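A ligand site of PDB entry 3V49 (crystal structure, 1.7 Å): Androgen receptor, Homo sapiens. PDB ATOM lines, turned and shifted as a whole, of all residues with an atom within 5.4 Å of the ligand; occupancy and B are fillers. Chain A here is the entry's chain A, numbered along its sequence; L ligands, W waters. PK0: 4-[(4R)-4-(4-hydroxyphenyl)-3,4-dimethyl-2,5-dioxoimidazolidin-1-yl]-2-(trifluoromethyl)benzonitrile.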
ATOM      1  N   LEU A  48     -10.822  16.922  36.880  1.00  0.00           N
ATOM      2  CA  LEU A  48     -12.237  17.143  36.506  1.00  0.00           C
ATOM      3  C   LEU A  48     -12.553  18.623  36.526  1.00  0.00           C
ATOM      4  O   LEU A  48     -13.345  19.081  35.704  1.00  0.00           O
ATOM      5  CB  LEU A  48     -13.195  16.385  37.411  1.00  0.00           C
ATOM      6  CG  LEU A  48     -14.692  16.343  37.085  1.00  0.00           C
ATOM      7  CD1 LEU A  48     -15.041  15.551  35.859  1.00  0.00           C
ATOM      8  CD2 LEU A  48     -15.366  15.830  38.379  1.00  0.00           C
ATOM      9  N   LEU A  51     -11.439  19.891  33.290  1.00  0.00           N
ATOM     10  CA  LEU A  51     -12.229  19.441  32.119  1.00  0.00           C
ATOM     11  C   LEU A  51     -13.554  20.191  32.063  1.00  0.00           C
ATOM     12  O   LEU A  51     -14.041  20.542  30.978  1.00  0.00           O
ATOM     13  CB  LEU A  51     -12.422  17.945  32.205  1.00  0.00           C
ATOM     14  CG  LEU A  51     -11.152  17.089  31.972  1.00  0.00           C
ATOM     15  CD1 LEU A  51     -11.412  15.702  32.498  1.00  0.00           C
ATOM     16  CD2 LEU A  51     -10.812  17.120  30.494  1.00  0.00           C
ATOM     17  N   ASN A  52     -14.133  20.417  33.233  1.00  0.00           N
ATOM     18  CA  ASN A  52     -15.339  21.223  33.315  1.00  0.00           C
ATOM     19  C   ASN A  52     -15.110  22.629  32.748  1.00  0.00           C
ATOM     20  O   ASN A  52     -15.884  23.182  31.949  1.00  0.00           O
ATOM     21  CB  ASN A  52     -15.829  21.346  34.782  1.00  0.00           C
ATOM     22  CG  ASN A  52     -16.822  20.250  35.138  1.00  0.00           C
ATOM     23  OD1 ASN A  52     -17.646  19.807  34.314  1.00  0.00           O
ATOM     24  ND2 ASN A  52     -16.795  19.773  36.387  1.00  0.00           N
ATOM     25  N   LEU A  54     -12.637  23.614  30.716  1.00  0.00           N
ATOM     26  CA  LEU A  54     -12.337  23.531  29.289  1.00  0.00           C
ATOM     27  C   LEU A  54     -13.612  23.317  28.474  1.00  0.00           C
ATOM     28  O   LEU A  54     -13.827  23.970  27.453  1.00  0.00           O
ATOM     29  CB  LEU A  54     -11.335  22.397  29.015  1.00  0.00           C
ATOM     30  CG  LEU A  54     -10.886  22.245  27.569  1.00  0.00           C
ATOM     31  CD1 LEU A  54     -10.238  23.520  27.020  1.00  0.00           C
ATOM     32  CD2 LEU A  54      -9.916  21.076  27.419  1.00  0.00           C
ATOM     33  N   GLY A  55     -14.426  22.400  28.971  1.00  0.00           N
ATOM     34  CA  GLY A  55     -15.696  22.052  28.365  1.00  0.00           C
ATOM     35  C   GLY A  55     -16.611  23.268  28.171  1.00  0.00           C
ATOM     36  O   GLY A  55     -17.192  23.501  27.104  1.00  0.00           O
ATOM     37  N   GLU A  56     -16.732  24.088  29.225  1.00  0.00           N
ATOM     38  CA  GLU A  56     -17.518  25.309  29.093  1.00  0.00           C
ATOM     39  C   GLU A  56     -16.889  26.291  28.127  1.00  0.00           C
ATOM     40  O   GLU A  56     -17.585  26.911  27.318  1.00  0.00           O
ATOM     41  CB  GLU A  56     -17.730  25.959  30.468  1.00  0.00           C
ATOM     42  CG  GLU A  56     -18.671  27.145  30.329  1.00  0.00           C
ATOM     43  CD  GLU A  56     -19.294  27.608  31.639  1.00  0.00           C
ATOM     44  OE1 GLU A  56     -19.102  26.923  32.650  1.00  0.00           O
ATOM     45  OE2 GLU A  56     -19.941  28.679  31.578  1.00  0.00           O
ATOM     46  N   GLN A  58     -14.987  25.660  25.571  1.00  0.00           N
ATOM     47  CA  GLN A  58     -15.164  25.190  24.203  1.00  0.00           C
ATOM     48  C   GLN A  58     -16.612  25.367  23.769  1.00  0.00           C
ATOM     49  O   GLN A  58     -16.879  25.685  22.595  1.00  0.00           O
ATOM     50  CB  GLN A  58     -14.733  23.721  24.069  1.00  0.00           C
ATOM     51  CG  GLN A  58     -13.222  23.509  24.054  1.00  0.00           C
ATOM     52  CD  GLN A  58     -12.523  23.803  22.762  1.00  0.00           C
ATOM     53  OE1 GLN A  58     -13.040  24.347  21.776  1.00  0.00           O
ATOM     54  NE2 GLN A  58     -11.241  23.416  22.717  1.00  0.00           N
ATOM     55  N   TRP A  88     -22.441  18.916  21.079  1.00  0.00           N
ATOM     56  CA  TRP A  88     -21.180  19.523  21.549  1.00  0.00           C
ATOM     57  C   TRP A  88     -20.134  18.503  21.974  1.00  0.00           C
ATOM     58  O   TRP A  88     -18.961  18.664  21.581  1.00  0.00           O
ATOM     59  CB  TRP A  88     -21.397  20.564  22.667  1.00  0.00           C
ATOM     60  CG  TRP A  88     -21.579  20.046  24.041  1.00  0.00           C
ATOM     61  CD1 TRP A  88     -22.684  19.258  24.314  1.00  0.00           C
ATOM     62  CD2 TRP A  88     -20.878  20.151  25.285  1.00  0.00           C
ATOM     63  NE1 TRP A  88     -22.697  18.868  25.624  1.00  0.00           N
ATOM     64  CE2 TRP A  88     -21.602  19.406  26.235  1.00  0.00           C
ATOM     65  CE3 TRP A  88     -19.700  20.769  25.740  1.00  0.00           C
ATOM     66  CZ2 TRP A  88     -21.233  19.248  27.575  1.00  0.00           C
ATOM     67  CZ3 TRP A  88     -19.344  20.623  27.065  1.00  0.00           C
ATOM     68  CH2 TRP A  88     -20.088  19.874  27.969  1.00  0.00           C
ATOM     69  N   MET A  89     -20.492  17.484  22.740  1.00  0.00           N
ATOM     70  CA  MET A  89     -19.435  16.524  23.147  1.00  0.00           C
ATOM     71  C   MET A  89     -18.837  15.861  21.911  1.00  0.00           C
ATOM     72  O   MET A  89     -17.622  15.669  21.828  1.00  0.00           O
ATOM     73  CB  MET A  89     -20.037  15.533  24.144  1.00  0.00           C
ATOM     74  CG  MET A  89     -19.051  14.709  24.967  1.00  0.00           C
ATOM     75  SD  MET A  89     -17.782  15.669  25.814  1.00  0.00           S
ATOM     76  CE  MET A  89     -18.865  16.800  26.738  1.00  0.00           C
ATOM     77  N   MET A  92     -16.390  18.154  20.351  1.00  0.00           N
ATOM     78  CA  MET A  92     -15.145  18.332  21.102  1.00  0.00           C
ATOM     79  C   MET A  92     -14.244  17.111  20.954  1.00  0.00           C
ATOM     80  O   MET A  92     -13.027  17.250  20.802  1.00  0.00           O
ATOM     81  CB  MET A  92     -15.398  18.632  22.587  1.00  0.00           C
ATOM     82  CG  MET A  92     -16.078  19.959  22.900  1.00  0.00           C
ATOM     83  SD  MET A  92     -15.813  20.359  24.661  1.00  0.00           S
ATOM     84  CE  MET A  92     -16.761  19.064  25.458  1.00  0.00           C
ATOM     85  N   VAL A  93     -14.842  15.916  20.953  1.00  0.00           N
ATOM     86  CA  VAL A  93     -14.062  14.689  20.748  1.00  0.00           C
ATOM     87  C   VAL A  93     -13.329  14.674  19.426  1.00  0.00           C
ATOM     88  O   VAL A  93     -12.122  14.380  19.382  1.00  0.00           O
ATOM     89  CB  VAL A  93     -15.005  13.477  20.853  1.00  0.00           C
ATOM     90  CG1 VAL A  93     -14.333  12.170  20.439  1.00  0.00           C
ATOM     91  CG2 VAL A  93     -15.455  13.380  22.314  1.00  0.00           C
ATOM     92  N   MET A  96     -10.555  17.312  19.358  1.00  0.00           N
ATOM     93  CA  MET A  96      -9.448  16.929  20.231  1.00  0.00           C
ATOM     94  C   MET A  96      -8.631  15.840  19.560  1.00  0.00           C
ATOM     95  O   MET A  96      -7.408  15.844  19.575  1.00  0.00           O
ATOM     96  CB  MET A  96      -9.948  16.524  21.628  1.00  0.00           C
ATOM     97  CG  MET A  96      -8.772  16.440  22.609  1.00  0.00           C
ATOM     98  SD  MET A  96      -8.028  14.795  22.599  1.00  0.00           S
ATOM     99  CE  MET A  96      -9.411  13.852  23.282  1.00  0.00           C
ATOM    100  N   ARG A  99      -6.467  17.527  16.973  1.00  0.00           N
ATOM    101  CA  ARG A  99      -5.324  18.231  17.560  1.00  0.00           C
ATOM    102  C   ARG A  99      -4.249  17.264  18.034  1.00  0.00           C
ATOM    103  O   ARG A  99      -3.055  17.570  17.923  1.00  0.00           O
ATOM    104  CB  ARG A  99      -5.699  19.071  18.779  1.00  0.00           C
ATOM    105  CG  ARG A  99      -6.555  20.298  18.464  1.00  0.00           C
ATOM    106  CD  ARG A  99      -6.667  21.157  19.721  1.00  0.00           C
ATOM    107  NE  ARG A  99      -7.395  20.534  20.825  1.00  0.00           N
ATOM    108  CZ  ARG A  99      -8.716  20.467  20.917  1.00  0.00           C
ATOM    109  NH1 ARG A  99      -9.487  20.986  19.958  1.00  0.00           N
ATOM    110  NH2 ARG A  99      -9.257  19.879  21.974  1.00  0.00           N
ATOM    111  N   PHE A 111      -5.858  17.802  24.795  1.00  0.00           N
ATOM    112  CA  PHE A 111      -7.107  18.491  25.134  1.00  0.00           C
ATOM    113  C   PHE A 111      -6.973  20.001  24.932  1.00  0.00           C
ATOM    114  O   PHE A 111      -7.807  20.674  24.363  1.00  0.00           O
ATOM    115  CB  PHE A 111      -7.522  18.218  26.593  1.00  0.00           C
ATOM    116  CG  PHE A 111      -8.124  16.841  26.822  1.00  0.00           C
ATOM    117  CD1 PHE A 111      -7.303  15.713  26.905  1.00  0.00           C
ATOM    118  CD2 PHE A 111      -9.480  16.664  26.977  1.00  0.00           C
ATOM    119  CE1 PHE A 111      -7.841  14.465  27.149  1.00  0.00           C
ATOM    120  CE2 PHE A 111     -10.024  15.412  27.209  1.00  0.00           C
ATOM    121  CZ  PHE A 111      -9.214  14.292  27.294  1.00  0.00           C
ATOM    122  N   MET A 127     -11.184   8.189  33.301  1.00  0.00           N
ATOM    123  CA  MET A 127     -11.770   8.010  31.975  1.00  0.00           C
ATOM    124  C   MET A 127     -10.822   7.236  31.068  1.00  0.00           C
ATOM    125  O   MET A 127     -10.694   7.543  29.874  1.00  0.00           O
ATOM    126  CB  MET A 127     -12.093   9.363  31.350  1.00  0.00           C
ATOM    127  CG  MET A 127     -12.746  10.408  32.247  1.00  0.00           C
ATOM    128  SD  MET A 127     -13.405  11.793  31.283  1.00  0.00           S
ATOM    129  CE  MET A 127     -11.948  12.496  30.529  1.00  0.00           C
ATOM    130  N   MET A 134     -10.306   7.533  22.249  1.00  0.00           N
ATOM    131  CA  MET A 134     -10.044   8.820  21.602  1.00  0.00           C
ATOM    132  C   MET A 134      -8.643   8.836  20.986  1.00  0.00           C
ATOM    133  O   MET A 134      -8.401   9.429  19.941  1.00  0.00           O
ATOM    134  CB  MET A 134     -10.252  10.014  22.555  1.00  0.00           C
ATOM    135  CG  MET A 134     -11.723  10.192  22.914  1.00  0.00           C
ATOM    136  SD  MET A 134     -12.087  11.689  23.840  1.00  0.00           S
ATOM    137  CE  MET A 134     -11.366  11.333  25.432  1.00  0.00           C
ATOM    138  N   LEU A 220     -18.588   9.340  27.394  1.00  0.00           N
ATOM    139  CA  LEU A 220     -18.265  10.505  28.207  1.00  0.00           C
ATOM    140  C   LEU A 220     -19.493  11.000  28.972  1.00  0.00           C
ATOM    141  O   LEU A 220     -19.377  11.321  30.168  1.00  0.00           O
ATOM    142  CB  LEU A 220     -17.678  11.623  27.342  1.00  0.00           C
ATOM    143  CG  LEU A 220     -16.289  11.262  26.775  1.00  0.00           C
ATOM    144  CD1 LEU A 220     -15.885  12.228  25.664  1.00  0.00           C
ATOM    145  CD2 LEU A 220     -15.243  11.217  27.874  1.00  0.00           C
ATOM    146  N   HIS A 221     -20.635  11.032  28.279  1.00  0.00           N
ATOM    147  CA  HIS A 221     -21.889  11.470  28.905  1.00  0.00           C
ATOM    148  C   HIS A 221     -22.270  10.553  30.054  1.00  0.00           C
ATOM    149  O   HIS A 221     -22.607  11.046  31.141  1.00  0.00           O
ATOM    150  CB  HIS A 221     -23.035  11.524  27.880  1.00  0.00           C
ATOM    151  CG  HIS A 221     -22.953  12.691  26.934  1.00  0.00           C
ATOM    152  ND1 HIS A 221     -22.542  13.934  27.336  1.00  0.00           N
ATOM    153  CD2 HIS A 221     -23.256  12.773  25.615  1.00  0.00           C
ATOM    154  CE1 HIS A 221     -22.581  14.762  26.295  1.00  0.00           C
ATOM    155  NE2 HIS A 221     -23.001  14.065  25.247  1.00  0.00           N
ATOM    156  N   PHE A 223     -20.383   8.493  31.883  1.00  0.00           N
ATOM    157  CA  PHE A 223     -19.452   8.660  32.992  1.00  0.00           C
ATOM    158  C   PHE A 223     -19.763   9.914  33.799  1.00  0.00           C
ATOM    159  O   PHE A 223     -19.743   9.940  35.037  1.00  0.00           O
ATOM    160  CB  PHE A 223     -18.026   8.688  32.417  1.00  0.00           C
ATOM    161  CG  PHE A 223     -16.978   9.265  33.370  1.00  0.00           C
ATOM    162  CD1 PHE A 223     -16.576  10.582  33.286  1.00  0.00           C
ATOM    163  CD2 PHE A 223     -16.416   8.424  34.334  1.00  0.00           C
ATOM    164  CE1 PHE A 223     -15.609  11.066  34.161  1.00  0.00           C
ATOM    165  CE2 PHE A 223     -15.476   8.916  35.218  1.00  0.00           C
ATOM    166  CZ  PHE A 223     -15.077  10.239  35.141  1.00  0.00           C
ATOM    167  N   THR A 224     -20.027  11.042  33.113  1.00  0.00           N
ATOM    168  CA  THR A 224     -20.229  12.300  33.813  1.00  0.00           C
ATOM    169  C   THR A 224     -21.598  12.432  34.468  1.00  0.00           C
ATOM    170  O   THR A 224     -21.764  12.979  35.565  1.00  0.00           O
ATOM    171  CB  THR A 224     -19.976  13.454  32.810  1.00  0.00           C
ATOM    172  OG1 THR A 224     -18.698  13.232  32.178  1.00  0.00           O
ATOM    173  CG2 THR A 224     -19.916  14.768  33.542  1.00  0.00           C
ATOM    174  N   MET A 242     -22.647  23.257  33.283  1.00  0.00           N
ATOM    175  CA  MET A 242     -22.467  21.807  33.102  1.00  0.00           C
ATOM    176  C   MET A 242     -23.586  21.050  33.819  1.00  0.00           C
ATOM    177  O   MET A 242     -24.146  20.077  33.323  1.00  0.00           O
ATOM    178  CB  MET A 242     -21.097  21.344  33.590  1.00  0.00           C
ATOM    179  CG  MET A 242     -19.912  21.962  32.852  1.00  0.00           C
ATOM    180  SD  MET A 242     -19.862  21.455  31.116  1.00  0.00           S
ATOM    181  CE  MET A 242     -20.753  22.744  30.274  1.00  0.00           C
ATOM    182  N   ILE A 245     -26.590  21.220  31.606  1.00  0.00           N
ATOM    183  CA  ILE A 245     -26.605  20.345  30.421  1.00  0.00           C
ATOM    184  C   ILE A 245     -26.611  18.889  30.808  1.00  0.00           C
ATOM    185  O   ILE A 245     -27.274  18.079  30.122  1.00  0.00           O
ATOM    186  CB  ILE A 245     -25.429  20.688  29.498  1.00  0.00           C
ATOM    187  CG1 ILE A 245     -25.526  22.135  29.023  1.00  0.00           C
ATOM    188  CG2 ILE A 245     -25.343  19.731  28.313  1.00  0.00           C
ATOM    189  CD1 ILE A 245     -24.295  22.508  28.178  1.00  0.00           C
ATOM    190  N   ILE A 246     -25.940  18.528  31.895  1.00  0.00           N
ATOM    191  CA  ILE A 246     -25.901  17.108  32.256  1.00  0.00           C
ATOM    192  C   ILE A 246     -27.253  16.640  32.789  1.00  0.00           C
ATOM    193  O   ILE A 246     -27.607  15.484  32.583  1.00  0.00           O
ATOM    194  CB  ILE A 246     -24.769  16.834  33.267  1.00  0.00           C
ATOM    195  CG1 ILE A 246     -23.384  17.218  32.667  1.00  0.00           C
ATOM    196  CG2 ILE A 246     -24.790  15.404  33.748  1.00  0.00           C
ATOM    197  CD1 ILE A 246     -22.382  17.484  33.790  1.00  0.00           C
ATOM    198  N   VAL A 250     -28.418  15.825  28.573  1.00  0.00           N
ATOM    199  CA  VAL A 250     -27.768  14.536  28.489  1.00  0.00           C
ATOM    200  C   VAL A 250     -28.696  13.352  28.781  1.00  0.00           C
ATOM    201  O   VAL A 250     -28.487  12.347  28.079  1.00  0.00           O
ATOM    202  CB  VAL A 250     -26.525  14.494  29.408  1.00  0.00           C
ATOM    203  CG1 VAL A 250     -25.946  13.098  29.533  1.00  0.00           C
ATOM    204  CG2 VAL A 250     -25.483  15.461  28.839  1.00  0.00           C
HETATM  205  N4  PK0 L   1     -15.878  15.786  30.921  1.00  0.00           N
HETATM  206  C31 PK0 L   1     -16.382  17.897  31.879  1.00  0.00           C
HETATM  207  C4  PK0 L   1     -15.909  14.740  31.964  1.00  0.00           C
HETATM  208  O2  PK0 L   1     -16.623  18.800  29.280  1.00  0.00           O
HETATM  209  C2  PK0 L   1     -16.228  17.755  29.666  1.00  0.00           C
HETATM  210  O5  PK0 L   1     -14.064  15.043  29.618  1.00  0.00           O
HETATM  211  C5  PK0 L   1     -14.887  15.876  29.901  1.00  0.00           C
HETATM  212  C3  PK0 L   1     -16.748  16.919  30.759  1.00  0.00           C
HETATM  213  C1B PK0 L   1     -18.181  16.625  30.436  1.00  0.00           C
HETATM  214  C2B PK0 L   1     -19.206  17.505  30.762  1.00  0.00           C
HETATM  215  C3B PK0 L   1     -20.513  17.141  30.439  1.00  0.00           C
HETATM  216  C4B PK0 L   1     -20.857  15.981  29.764  1.00  0.00           C
HETATM  217  C5B PK0 L   1     -19.805  15.109  29.457  1.00  0.00           C
HETATM  218  C6B PK0 L   1     -18.496  15.436  29.784  1.00  0.00           C
HETATM  219  O4  PK0 L   1     -22.190  15.655  29.481  1.00  0.00           O
HETATM  220  N1  PK0 L   1     -15.054  17.160  29.328  1.00  0.00           N
HETATM  221  C1A PK0 L   1     -14.299  17.443  28.176  1.00  0.00           C
HETATM  222  C2A PK0 L   1     -13.782  18.750  28.011  1.00  0.00           C
HETATM  223  C3A PK0 L   1     -13.044  19.120  26.902  1.00  0.00           C
HETATM  224  C4A PK0 L   1     -12.785  18.151  25.919  1.00  0.00           C
HETATM  225  C5A PK0 L   1     -13.277  16.876  26.054  1.00  0.00           C
HETATM  226  C6A PK0 L   1     -14.029  16.520  27.173  1.00  0.00           C
HETATM  227  C41 PK0 L   1     -11.893  18.576  24.786  1.00  0.00           C
HETATM  228  N41 PK0 L   1     -11.266  19.158  23.905  1.00  0.00           N
HETATM  229  C51 PK0 L   1     -13.009  15.910  24.977  1.00  0.00           C
HETATM  230  F1  PK0 L   1     -11.872  15.867  24.493  1.00  0.00           F
HETATM  231  F2  PK0 L   1     -13.666  15.988  23.926  1.00  0.00           F
HETATM  232  F3  PK0 L   1     -13.126  14.695  25.214  1.00  0.00           F
HETATM  233  O   HOH W   1     -12.148  20.020  21.122  1.00  0.00           O
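NH2 of Arg 99 is in hydrogen-bond range of O of Phe 111, at 2.9 Å. OG1 of Thr 224 is in hydrogen-bond range of O of Leu 220, 2.9 Å away. The backbone carbonyl oxygen (O) of Ile 245 is in hydrogen-bond range of the backbone NH (N) of Val 250 (3.0 Å).
Water W1 lies within hydrogen-bond range of the backbone carbonyl oxygen of Met 92 (2.9 Å), the guanidinium group of Arg 99 (3.0 Å) and a nitrogen (N41) of the ligand (3.0 Å).
O of Met 92 lies close to F2 of the ligand, at 3.4 Å. The backbone NH (N) of Val 93 sits close to a fluorine (F2) of the ligand (3.2 Å). An oxygen (O5) of the ligand lies close to the side-chain sulfur (SD) of Met 127 (3.7 Å). SD of Met 134 sits close to F3 of the ligand (3.5 Å). Residues that only touch the ligand: Leu 51, Asn 52, Leu 54, Gly 55, Trp 88, Met 89, Met 96, Phe 111, Leu 220, Thr 224, Ile 246 and Val 250. Hydrophobic or aromatic side chains that line the ligand: Leu 51, Leu 54, Trp 88, Met 89, Met 92, Val 93, Met 96, Phe 111, Met 127, Met 134, Leu 220, His 221, Ile 246 and Val 250. Of the 24 residues printed, 18 come within 4 Å of the ligand.
ND1 of His 221 is in hydrogen-bond range of O4 of the ligand. The guanidinium group (NH2) of Arg 99 lies within hydrogen-bond range of a nitrogen (N41) of the ligand.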
